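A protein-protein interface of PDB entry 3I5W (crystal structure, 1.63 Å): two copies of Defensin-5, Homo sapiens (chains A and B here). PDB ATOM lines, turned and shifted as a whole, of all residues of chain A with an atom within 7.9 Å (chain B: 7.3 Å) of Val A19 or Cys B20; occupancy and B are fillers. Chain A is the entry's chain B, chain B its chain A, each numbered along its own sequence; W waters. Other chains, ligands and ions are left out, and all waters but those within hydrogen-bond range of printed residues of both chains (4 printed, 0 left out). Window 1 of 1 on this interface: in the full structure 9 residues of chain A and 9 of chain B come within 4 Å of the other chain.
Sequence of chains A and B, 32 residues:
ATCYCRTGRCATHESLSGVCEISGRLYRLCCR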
ATOM      1  N   CYS A   3       5.322  -0.347  -7.867  1.00  0.00           N
ATOM      2  CA  CYS A   3       5.136  -0.749  -9.248  1.00  0.00           C
ATOM      3  C   CYS A   3       3.673  -0.761  -9.619  1.00  0.00           C
ATOM      4  O   CYS A   3       2.768  -0.842  -8.751  1.00  0.00           O
ATOM      5  CB  CYS A   3       5.703  -2.154  -9.506  1.00  0.00           C
ATOM      6  SG  CYS A   3       7.355  -2.418  -8.884  1.00  0.00           S
ATOM      7  N   TYR A   4       3.466  -0.652 -10.919  1.00  0.00           N
ATOM      8  CA  TYR A   4       2.164  -0.692 -11.511  1.00  0.00           C
ATOM      9  C   TYR A   4       2.200  -1.611 -12.684  1.00  0.00           C
ATOM     10  O   TYR A   4       3.163  -1.650 -13.426  1.00  0.00           O
ATOM     11  CB  TYR A   4       1.742   0.722 -11.962  1.00  0.00           C
ATOM     12  CG  TYR A   4       1.968   1.767 -10.910  1.00  0.00           C
ATOM     13  CD1 TYR A   4       3.173   2.451 -10.865  1.00  0.00           C
ATOM     14  CD2 TYR A   4       0.993   2.054  -9.957  1.00  0.00           C
ATOM     15  CE1 TYR A   4       3.425   3.437  -9.890  1.00  0.00           C
ATOM     16  CE2 TYR A   4       1.228   3.037  -8.977  1.00  0.00           C
ATOM     17  CZ  TYR A   4       2.445   3.707  -8.958  1.00  0.00           C
ATOM     18  OH  TYR A   4       2.696   4.678  -8.012  1.00  0.00           O
ATOM     19  N   CYS A   5       1.124  -2.390 -12.820  1.00  0.00           N
ATOM     20  CA  CYS A   5       0.910  -3.227 -13.962  1.00  0.00           C
ATOM     21  C   CYS A   5       0.181  -2.360 -14.952  1.00  0.00           C
ATOM     22  O   CYS A   5      -1.013  -1.970 -14.730  1.00  0.00           O
ATOM     23  CB  CYS A   5       0.005  -4.402 -13.528  1.00  0.00           C
ATOM     24  SG  CYS A   5       0.855  -5.494 -12.316  1.00  0.00           S
ATOM     25  N   LEU A  16      10.922  -0.692 -16.660  1.00  0.00           N
ATOM     26  CA  LEU A  16      10.198  -1.898 -16.992  1.00  0.00           C
ATOM     27  C   LEU A  16      10.916  -3.023 -16.263  1.00  0.00           C
ATOM     28  O   LEU A  16      12.120  -3.217 -16.422  1.00  0.00           O
ATOM     29  CB  LEU A  16      10.269  -2.162 -18.512  1.00  0.00           C
ATOM     30  CG  LEU A  16       9.542  -3.436 -18.941  1.00  0.00           C
ATOM     31  CD1 LEU A  16       8.041  -3.423 -18.652  1.00  0.00           C
ATOM     32  CD2 LEU A  16       9.794  -3.692 -20.438  1.00  0.00           C
ATOM     33  N   SER A  17      10.156  -3.734 -15.436  1.00  0.00           N
ATOM     34  CA  SER A  17      10.787  -4.662 -14.517  1.00  0.00           C
ATOM     35  C   SER A  17      10.312  -6.087 -14.622  1.00  0.00           C
ATOM     36  O   SER A  17      10.868  -6.982 -13.931  1.00  0.00           O
ATOM     37  CB  SER A  17      10.558  -4.188 -13.058  1.00  0.00           C
ATOM     38  OG  SER A  17      11.052  -2.868 -12.870  1.00  0.00           O
ATOM     39  N   GLY A  18       9.324  -6.350 -15.469  1.00  0.00           N
ATOM     40  CA  GLY A  18       8.742  -7.674 -15.523  1.00  0.00           C
ATOM     41  C   GLY A  18       7.408  -7.597 -16.227  1.00  0.00           C
ATOM     42  O   GLY A  18       7.109  -6.606 -16.934  1.00  0.00           O
ATOM     43  N   VAL A  19       6.595  -8.622 -15.947  1.00  0.00           N
ATOM     44  CA  VAL A  19       5.276  -8.808 -16.583  1.00  0.00           C
ATOM     45  C   VAL A  19       4.269  -9.151 -15.485  1.00  0.00           C
ATOM     46  O   VAL A  19       4.576  -9.951 -14.630  1.00  0.00           O
ATOM     47  CB  VAL A  19       5.328  -9.974 -17.604  1.00  0.00           C
ATOM     48  CG1 VAL A  19       3.955 -10.323 -18.154  1.00  0.00           C
ATOM     49  CG2 VAL A  19       6.264  -9.625 -18.750  1.00  0.00           C
ATOM     50  N   CYS A  20       3.089  -8.531 -15.493  1.00  0.00           N
ATOM     51  CA  CYS A  20       1.970  -9.009 -14.675  1.00  0.00           C
ATOM     52  C   CYS A  20       0.999  -9.783 -15.570  1.00  0.00           C
ATOM     53  O   CYS A  20       0.693  -9.387 -16.703  1.00  0.00           O
ATOM     54  CB  CYS A  20       1.147  -7.874 -14.053  1.00  0.00           C
ATOM     55  SG  CYS A  20       2.195  -6.535 -13.392  1.00  0.00           S
ATOM     56  N   GLU A  21       0.496 -10.865 -15.032  1.00  0.00           N
ATOM     57  CA  GLU A  21      -0.634 -11.559 -15.647  1.00  0.00           C
ATOM     58  C   GLU A  21      -1.837 -11.354 -14.717  1.00  0.00           C
ATOM     59  O   GLU A  21      -1.835 -11.778 -13.532  1.00  0.00           O
ATOM     60  CB  GLU A  21      -0.346 -13.044 -15.848  1.00  0.00           C
ATOM     61  CG  GLU A  21      -1.639 -13.756 -16.380  1.00  0.00           C
ATOM     62  CD  GLU A  21      -1.497 -15.256 -16.673  1.00  0.00           C
ATOM     63  OE1 GLU A  21      -0.395 -15.790 -16.606  1.00  0.00           O
ATOM     64  OE2 GLU A  21      -2.529 -15.866 -17.004  1.00  0.00           O
ATOM     65  N   ILE A  22      -2.912 -10.735 -15.240  1.00  0.00           N
ATOM     66  CA  ILE A  22      -4.095 -10.475 -14.447  1.00  0.00           C
ATOM     67  C   ILE A  22      -5.279 -10.843 -15.312  1.00  0.00           C
ATOM     68  O   ILE A  22      -5.409 -10.266 -16.390  1.00  0.00           O
ATOM     69  CB  ILE A  22      -4.218  -8.967 -14.075  1.00  0.00           C
ATOM     70  CG1 ILE A  22      -2.956  -8.465 -13.326  1.00  0.00           C
ATOM     71  CG2 ILE A  22      -5.443  -8.760 -13.230  1.00  0.00           C
ATOM     72  CD1 ILE A  22      -2.896  -6.930 -13.253  1.00  0.00           C
ATOM     73  N   ARG A  25      -4.764 -11.466 -19.176  1.00  0.00           N
ATOM     74  CA  ARG A  25      -4.087 -10.473 -19.969  1.00  0.00           C
ATOM     75  C   ARG A  25      -2.722 -10.229 -19.354  1.00  0.00           C
ATOM     76  O   ARG A  25      -2.570 -10.306 -18.115  1.00  0.00           O
ATOM     77  CB  ARG A  25      -4.920  -9.180 -19.949  1.00  0.00           C
ATOM     78  CG  ARG A  25      -6.186  -9.310 -20.814  1.00  0.00           C
ATOM     79  CD  ARG A  25      -6.887  -7.953 -20.940  1.00  0.00           C
ATOM     80  NE  ARG A  25      -6.027  -6.891 -21.496  1.00  0.00           N
ATOM     81  CZ  ARG A  25      -6.362  -5.596 -21.487  1.00  0.00           C
ATOM     82  NH1 ARG A  25      -7.524  -5.215 -20.935  1.00  0.00           N
ATOM     83  NH2 ARG A  25      -5.536  -4.680 -22.009  1.00  0.00           N
ATOM     84  N   LEU A  26      -1.748  -9.906 -20.211  1.00  0.00           N
ATOM     85  CA  LEU A  26      -0.427  -9.523 -19.754  1.00  0.00           C
ATOM     86  C   LEU A  26      -0.263  -8.004 -19.757  1.00  0.00           C
ATOM     87  O   LEU A  26      -0.773  -7.283 -20.644  1.00  0.00           O
ATOM     88  CB  LEU A  26       0.662 -10.188 -20.625  1.00  0.00           C
ATOM     89  CG  LEU A  26       0.521 -11.707 -20.698  1.00  0.00           C
ATOM     90  CD1 LEU A  26       1.520 -12.254 -21.733  1.00  0.00           C
ATOM     91  CD2 LEU A  26       0.746 -12.374 -19.316  1.00  0.00           C
ATOM     92  N   TYR A  27       0.511  -7.536 -18.781  1.00  0.00           N
ATOM     93  CA  TYR A  27       0.743  -6.115 -18.538  1.00  0.00           C
ATOM     94  C   TYR A  27       2.211  -5.908 -18.261  1.00  0.00           C
ATOM     95  O   TYR A  27       2.918  -6.820 -17.787  1.00  0.00           O
ATOM     96  CB  TYR A  27      -0.067  -5.606 -17.340  1.00  0.00           C
ATOM     97  CG  TYR A  27      -1.543  -5.781 -17.523  1.00  0.00           C
ATOM     98  CD1 TYR A  27      -2.194  -6.953 -17.116  1.00  0.00           C
ATOM     99  CD2 TYR A  27      -2.297  -4.767 -18.108  1.00  0.00           C
ATOM    100  CE1 TYR A  27      -3.564  -7.106 -17.306  1.00  0.00           C
ATOM    101  CE2 TYR A  27      -3.652  -4.907 -18.303  1.00  0.00           C
ATOM    102  CZ  TYR A  27      -4.301  -6.070 -17.863  1.00  0.00           C
ATOM    103  OH  TYR A  27      -5.672  -6.192 -18.075  1.00  0.00           O
ATOM    104  N   ARG A  28       2.699  -4.723 -18.598  1.00  0.00           N
ATOM    105  CA  ARG A  28       4.061  -4.400 -18.211  1.00  0.00           C
ATOM    106  C   ARG A  28       4.100  -4.098 -16.707  1.00  0.00           C
ATOM    107  O   ARG A  28       3.219  -3.380 -16.172  1.00  0.00           O
ATOM    108  CB  ARG A  28       4.492  -3.136 -18.930  1.00  0.00           C
ATOM    109  CG  ARG A  28       4.675  -3.257 -20.397  1.00  0.00           C
ATOM    110  CD  ARG A  28       4.763  -1.859 -21.025  1.00  0.00           C
ATOM    111  NE  ARG A  28       4.859  -2.026 -22.468  1.00  0.00           N
ATOM    112  CZ  ARG A  28       3.829  -2.135 -23.310  1.00  0.00           C
ATOM    113  NH1 ARG A  28       2.560  -2.070 -22.880  1.00  0.00           N
ATOM    114  NH2 ARG A  28       4.072  -2.304 -24.605  1.00  0.00           N
ATOM    115  N   LEU A  29       5.107  -4.609 -16.009  1.00  0.00           N
ATOM    116  CA  LEU A  29       5.353  -4.183 -14.612  1.00  0.00           C
ATOM    117  C   LEU A  29       6.341  -3.024 -14.633  1.00  0.00           C
ATOM    118  O   LEU A  29       7.497  -3.212 -14.991  1.00  0.00           O
ATOM    119  CB  LEU A  29       5.949  -5.365 -13.822  1.00  0.00           C
ATOM    120  CG  LEU A  29       6.278  -5.103 -12.352  1.00  0.00           C
ATOM    121  CD1 LEU A  29       4.948  -4.910 -11.593  1.00  0.00           C
ATOM    122  CD2 LEU A  29       7.136  -6.220 -11.748  1.00  0.00           C
ATOM    123  N   CYS A  30       5.862  -1.845 -14.241  1.00  0.00           N
ATOM    124  CA  CYS A  30       6.633  -0.606 -14.370  1.00  0.00           C
ATOM    125  C   CYS A  30       6.859  -0.150 -12.976  1.00  0.00           C
ATOM    126  O   CYS A  30       5.888   0.095 -12.234  1.00  0.00           O
ATOM    127  CB  CYS A  30       5.824   0.499 -15.134  1.00  0.00           C
ATOM    128  SG  CYS A  30       5.428   0.029 -16.805  1.00  0.00           S
ATOM    129  N   CYS B   3      -0.778  -2.763  -5.806  1.00  0.00           N
ATOM    130  CA  CYS B   3      -0.380  -4.177  -5.807  1.00  0.00           C
ATOM    131  C   CYS B   3       1.098  -4.318  -5.570  1.00  0.00           C
ATOM    132  O   CYS B   3       1.869  -3.367  -5.761  1.00  0.00           O
ATOM    133  CB  CYS B   3      -0.693  -4.801  -7.154  1.00  0.00           C
ATOM    134  SG  CYS B   3      -2.402  -4.644  -7.749  1.00  0.00           S
ATOM    135  N   TYR B   4       1.459  -5.512  -5.101  1.00  0.00           N
ATOM    136  CA  TYR B   4       2.834  -5.903  -4.823  1.00  0.00           C
ATOM    137  C   TYR B   4       3.107  -7.258  -5.376  1.00  0.00           C
ATOM    138  O   TYR B   4       2.250  -8.164  -5.270  1.00  0.00           O
ATOM    139  CB  TYR B   4       3.118  -5.876  -3.320  1.00  0.00           C
ATOM    140  CG  TYR B   4       2.859  -4.547  -2.734  1.00  0.00           C
ATOM    141  CD1 TYR B   4       1.644  -4.276  -2.152  1.00  0.00           C
ATOM    142  CD2 TYR B   4       3.837  -3.537  -2.820  1.00  0.00           C
ATOM    143  CE1 TYR B   4       1.389  -2.994  -1.612  1.00  0.00           C
ATOM    144  CE2 TYR B   4       3.611  -2.268  -2.303  1.00  0.00           C
ATOM    145  CZ  TYR B   4       2.381  -2.001  -1.708  1.00  0.00           C
ATOM    146  OH  TYR B   4       2.182  -0.720  -1.207  1.00  0.00           O
ATOM    147  N   CYS B   5       4.276  -7.424  -5.975  1.00  0.00           N
ATOM    148  CA  CYS B   5       4.725  -8.730  -6.432  1.00  0.00           C
ATOM    149  C   CYS B   5       5.496  -9.358  -5.304  1.00  0.00           C
ATOM    150  O   CYS B   5       6.615  -8.915  -4.992  1.00  0.00           O
ATOM    151  CB  CYS B   5       5.636  -8.570  -7.668  1.00  0.00           C
ATOM    152  SG  CYS B   5       4.775  -7.953  -9.160  1.00  0.00           S
ATOM    153  N   ARG B   6       4.847 -10.338  -4.671  1.00  0.00           N
ATOM    154  CA  ARG B   6       5.328 -10.968  -3.425  1.00  0.00           C
ATOM    155  C   ARG B   6       5.949 -12.322  -3.639  1.00  0.00           C
ATOM    156  O   ARG B   6       5.433 -13.189  -4.356  1.00  0.00           O
ATOM    157  CB  ARG B   6       4.204 -11.084  -2.369  1.00  0.00           C
ATOM    158  CG  ARG B   6       3.555  -9.739  -2.098  1.00  0.00           C
ATOM    159  CD  ARG B   6       2.971  -9.790  -0.717  1.00  0.00           C
ATOM    160  NE  ARG B   6       2.324  -8.535  -0.309  1.00  0.00           N
ATOM    161  CZ  ARG B   6       3.000  -7.450   0.135  1.00  0.00           C
ATOM    162  NH1 ARG B   6       4.336  -7.429   0.198  1.00  0.00           N
ATOM    163  NH2 ARG B   6       2.327  -6.332   0.480  1.00  0.00           N
ATOM    164  N   GLY B  18      -3.365 -12.052  -9.472  1.00  0.00           N
ATOM    165  CA  GLY B  18      -2.627 -12.577 -10.625  1.00  0.00           C
ATOM    166  C   GLY B  18      -1.230 -12.959 -10.210  1.00  0.00           C
ATOM    167  O   GLY B  18      -0.981 -13.270  -9.034  1.00  0.00           O
ATOM    168  N   VAL B  19      -0.312 -12.966 -11.169  1.00  0.00           N
ATOM    169  CA  VAL B  19       1.098 -13.307 -10.888  1.00  0.00           C
ATOM    170  C   VAL B  19       2.010 -12.289 -11.568  1.00  0.00           C
ATOM    171  O   VAL B  19       1.567 -11.582 -12.493  1.00  0.00           O
ATOM    172  CB  VAL B  19       1.489 -14.745 -11.341  1.00  0.00           C
ATOM    173  CG1 VAL B  19       0.715 -15.789 -10.457  1.00  0.00           C
ATOM    174  CG2 VAL B  19       1.147 -14.935 -12.845  1.00  0.00           C
ATOM    175  N   CYS B  20       3.244 -12.212 -11.081  1.00  0.00           N
ATOM    176  CA  CYS B  20       4.273 -11.400 -11.764  1.00  0.00           C
ATOM    177  C   CYS B  20       5.377 -12.355 -12.249  1.00  0.00           C
ATOM    178  O   CYS B  20       5.764 -13.335 -11.547  1.00  0.00           O
ATOM    179  CB  CYS B  20       4.948 -10.432 -10.804  1.00  0.00           C
ATOM    180  SG  CYS B  20       3.691  -9.554  -9.829  1.00  0.00           S
ATOM    181  N   GLU B  21       5.958 -12.009 -13.370  1.00  0.00           N
ATOM    182  CA  GLU B  21       7.166 -12.663 -13.872  1.00  0.00           C
ATOM    183  C   GLU B  21       8.256 -11.630 -13.759  1.00  0.00           C
ATOM    184  O   GLU B  21       8.186 -10.543 -14.390  1.00  0.00           O
ATOM    185  CB  GLU B  21       7.034 -13.056 -15.347  1.00  0.00           C
ATOM    186  CG  GLU B  21       5.746 -13.797 -15.702  1.00  0.00           C
ATOM    187  CD  GLU B  21       5.663 -14.092 -17.201  1.00  0.00           C
ATOM    188  OE1 GLU B  21       6.421 -13.495 -18.024  1.00  0.00           O
ATOM    189  OE2 GLU B  21       4.756 -14.873 -17.580  1.00  0.00           O
ATOM    190  N   ILE B  22       9.250 -11.925 -12.939  1.00  0.00           N
ATOM    191  CA  ILE B  22      10.381 -11.017 -12.775  1.00  0.00           C
ATOM    192  C   ILE B  22      11.686 -11.795 -12.825  1.00  0.00           C
ATOM    193  O   ILE B  22      11.924 -12.687 -11.977  1.00  0.00           O
ATOM    194  CB  ILE B  22      10.299 -10.273 -11.425  1.00  0.00           C
ATOM    195  CG1 ILE B  22       8.979  -9.502 -11.295  1.00  0.00           C
ATOM    196  CG2 ILE B  22      11.508  -9.326 -11.261  1.00  0.00           C
ATOM    197  CD1 ILE B  22       8.742  -8.935  -9.861  1.00  0.00           C
ATOM    198  N   SER B  23      12.490 -11.485 -13.822  1.00  0.00           N
ATOM    199  CA  SER B  23      13.819 -12.132 -13.927  1.00  0.00           C
ATOM    200  C   SER B  23      13.767 -13.655 -13.817  1.00  0.00           C
ATOM    201  O   SER B  23      14.576 -14.235 -13.108  1.00  0.00           O
ATOM    202  CB  SER B  23      14.757 -11.572 -12.853  1.00  0.00           C
ATOM    203  OG  SER B  23      15.050 -10.256 -13.230  1.00  0.00           O
ATOM    204  N   ARG B  25      11.523 -15.679 -12.464  1.00  0.00           N
ATOM    205  CA  ARG B  25      10.860 -16.202 -11.276  1.00  0.00           C
ATOM    206  C   ARG B  25       9.432 -15.695 -11.208  1.00  0.00           C
ATOM    207  O   ARG B  25       9.142 -14.602 -11.700  1.00  0.00           O
ATOM    208  CB  ARG B  25      11.662 -15.766 -10.031  1.00  0.00           C
ATOM    209  CG  ARG B  25      11.020 -16.028  -8.713  1.00  0.00           C
ATOM    210  CD  ARG B  25      11.945 -15.500  -7.570  1.00  0.00           C
ATOM    211  NE  ARG B  25      11.375 -15.920  -6.276  1.00  0.00           N
ATOM    212  CZ  ARG B  25      12.013 -15.948  -5.113  1.00  0.00           C
ATOM    213  NH1 ARG B  25      13.280 -15.548  -5.022  1.00  0.00           N
ATOM    214  NH2 ARG B  25      11.344 -16.379  -4.022  1.00  0.00           N
ATOM    215  N   LEU B  26       8.543 -16.535 -10.657  1.00  0.00           N
ATOM    216  CA  LEU B  26       7.134 -16.195 -10.502  1.00  0.00           C
ATOM    217  C   LEU B  26       6.863 -15.674  -9.090  1.00  0.00           C
ATOM    218  O   LEU B  26       7.398 -16.200  -8.075  1.00  0.00           O
ATOM    219  CB  LEU B  26       6.249 -17.432 -10.740  1.00  0.00           C
ATOM    220  CG  LEU B  26       4.764 -17.166 -11.037  1.00  0.00           C
ATOM    221  CD1 LEU B  26       4.598 -16.581 -12.508  1.00  0.00           C
ATOM    222  CD2 LEU B  26       3.930 -18.484 -10.867  1.00  0.00           C
ATOM    223  N   TYR B  27       6.015 -14.659  -9.032  1.00  0.00           N
ATOM    224  CA  TYR B  27       5.638 -13.974  -7.769  1.00  0.00           C
ATOM    225  C   TYR B  27       4.117 -13.898  -7.739  1.00  0.00           C
ATOM    226  O   TYR B  27       3.466 -13.889  -8.795  1.00  0.00           O
ATOM    227  CB  TYR B  27       6.152 -12.524  -7.776  1.00  0.00           C
ATOM    228  CG  TYR B  27       7.616 -12.397  -7.769  1.00  0.00           C
ATOM    229  CD1 TYR B  27       8.377 -12.717  -8.881  1.00  0.00           C
ATOM    230  CD2 TYR B  27       8.242 -11.887  -6.633  1.00  0.00           C
ATOM    231  CE1 TYR B  27       9.739 -12.624  -8.826  1.00  0.00           C
ATOM    232  CE2 TYR B  27       9.579 -11.752  -6.583  1.00  0.00           C
ATOM    233  CZ  TYR B  27      10.335 -12.095  -7.693  1.00  0.00           C
ATOM    234  OH  TYR B  27      11.734 -11.936  -7.614  1.00  0.00           O
ATOM    235  N   ARG B  28       3.550 -13.872  -6.528  1.00  0.00           N
ATOM    236  CA  ARG B  28       2.114 -13.567  -6.365  1.00  0.00           C
ATOM    237  C   ARG B  28       1.900 -12.071  -6.647  1.00  0.00           C
ATOM    238  O   ARG B  28       2.662 -11.247  -6.150  1.00  0.00           O
ATOM    239  CB  ARG B  28       1.640 -13.892  -4.962  1.00  0.00           C
ATOM    240  CG  ARG B  28       1.374 -15.374  -4.741  1.00  0.00           C
ATOM    241  CD  ARG B  28       0.948 -15.579  -3.335  1.00  0.00           C
ATOM    242  NE  ARG B  28       0.431 -16.916  -2.968  1.00  0.00           N
ATOM    243  CZ  ARG B  28       1.127 -17.891  -2.376  1.00  0.00           C
ATOM    244  NH1 ARG B  28       2.452 -17.777  -2.111  1.00  0.00           N
ATOM    245  NH2 ARG B  28       0.470 -18.975  -2.002  1.00  0.00           N
ATOM    246  N   LEU B  29       0.849 -11.737  -7.382  1.00  0.00           N
ATOM    247  CA  LEU B  29       0.403 -10.327  -7.473  1.00  0.00           C
ATOM    248  C   LEU B  29      -0.696 -10.129  -6.464  1.00  0.00           C
ATOM    249  O   LEU B  29      -1.820 -10.627  -6.633  1.00  0.00           O
ATOM    250  CB  LEU B  29      -0.072  -9.991  -8.897  1.00  0.00           C
ATOM    251  CG  LEU B  29      -0.467  -8.501  -9.032  1.00  0.00           C
ATOM    252  CD1 LEU B  29       0.787  -7.578  -9.045  1.00  0.00           C
ATOM    253  CD2 LEU B  29      -1.279  -8.348 -10.285  1.00  0.00           C
ATOM    254  N   CYS B  30      -0.353  -9.445  -5.381  1.00  0.00           N
ATOM    255  CA  CYS B  30      -1.242  -9.210  -4.223  1.00  0.00           C
ATOM    256  C   CYS B  30      -1.728  -7.761  -4.242  1.00  0.00           C
ATOM    257  O   CYS B  30      -0.931  -6.813  -4.227  1.00  0.00           O
ATOM    258  CB  CYS B  30      -0.531  -9.486  -2.897  1.00  0.00           C
ATOM    259  SG  CYS B  30       0.107 -11.183  -2.784  1.00  0.00           S
HETATM  260  O   HOH W   1      12.034  -9.362 -15.579  1.00  0.00           O
HETATM  261  O   HOH W   2       4.642  -2.837  -6.199  1.00  0.00           O
HETATM  262  O   HOH W   3      -0.004  -1.432  -8.300  1.00  0.00           O
HETATM  263  O   HOH W   4       2.250  -0.431  -5.871  1.00  0.00           O
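The backbone carbonyl oxygen (O) of Val B19 sits at hydrogen-bond distance from the backbone NH (N) of Glu A21 (2.8 Å). O of Val A19 lies within hydrogen-bond range of N of Glu B21 (2.8 Å).
Of the 16 printed residues of chain B, 7 touch a printed residue of chain A. Printed residues of chain B that touch a printed residue of chain A: Cys B5, Gly B18, Val B19, Cys B20, Glu B21, Ile B22 and Leu B29. Hydrophobic or aromatic side chains of chain B within 4 Å of the printed part of chain A: Val B19, Ile B22 and Leu B29. Along chain A the printed residues that touch a printed residue of chain B span positions 5 to 29. Among the printed residues, no Asp or Glu carboxylate lies within 4 Å of a Lys or Arg side-chain nitrogen of the other chain.
Val A19 touches two residues of chain B. Cys B20 touches just one residue of chain A: Val A19. Of the printed residues of chain A, Glu B21 touches Gly A18 (3.1 Å) and Val A19 (2.8 Å). Of the printed residues of chain A, Leu B29 touches Cys A5 (3.9 Å) and Ile A22 (3.5 Å). The nearest residue of chain B that does not touch Val A19 is Val B19 (4.03 Å). The nearest printed residue of chain B that does not touch Cys A5 is Cys B3 (5.4 Å).
Water W1 bridges N of Ser B23 (2.8 Å) and O of Ser A17 (3.1 Å). Water W2 bridges the backbone carbonyl oxygen (O) of Cys B3 and the backbone NH (N) of Cys A3. Water W3 lies within hydrogen-bond range of the backbone carbonyl oxygen of Cys A3 (2.9 Å) and the backbone NH of Cys B3 (2.9 Å). Water W4 bridges the backbone carbonyl oxygen (O) of Cys A3 (3.0 Å) and the backbone carbonyl oxygen (O) of Cys B3 (3.0 Å).
Among the printed residues, pairs that only touch across the chains: Glu A21 with Gly B18 (3.1 Å), Gly A18 with Glu B21 (3.1 Å), Val A19 with Cys B20 (3.2 Å), Cys A20 with Val B19 (3.4 Å), Ile A22 with Leu B29 (3.5 Å), Ser A17 with Ile B22 (3.6 Å), Leu A29 with Ile B22 (3.7 Å), Cys A5 with Leu B29 (3.9 Å) and Leu A29 with Cys B5 (3.9 Å).
Cys A5 touches Leu B29, and with the chains exchanged Leu A29 touches Cys B5. Gly A18 touches Glu B21, and with the chains exchanged Glu A21 touches Gly B18. Val A19 touches Cys B20, and with the chains exchanged Cys A20 touches Val B19. Ile A22 touches Leu B29, and with the chains exchanged Leu A29 touches Ile B22. Of the 11 pairs that touch across the chains among the printed residues, 10 have their exchanged pair printed and touching as well.
SG of Cys B5 forms a disulfide with SG of Cys B20 (2.0 Å). The backbone NH (N) of Cys B20 is in hydrogen-bond range of the backbone carbonyl oxygen (O) of Tyr B27 (2.8 Å). O of Cys A20 is in hydrogen-bond range of N of Tyr A27 (2.8 Å). The backbone NH (N) of Ser A17 sits at hydrogen-bond distance from the backbone carbonyl oxygen (O) of Leu A29 (2.7 Å). N of Leu A29 sits at hydrogen-bond distance from O of Gly A18 (3.0 Å). The backbone NH (N) of Leu B29 is in hydrogen-bond range of the backbone carbonyl oxygen (O) of Gly B18, 2.9 Å away.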
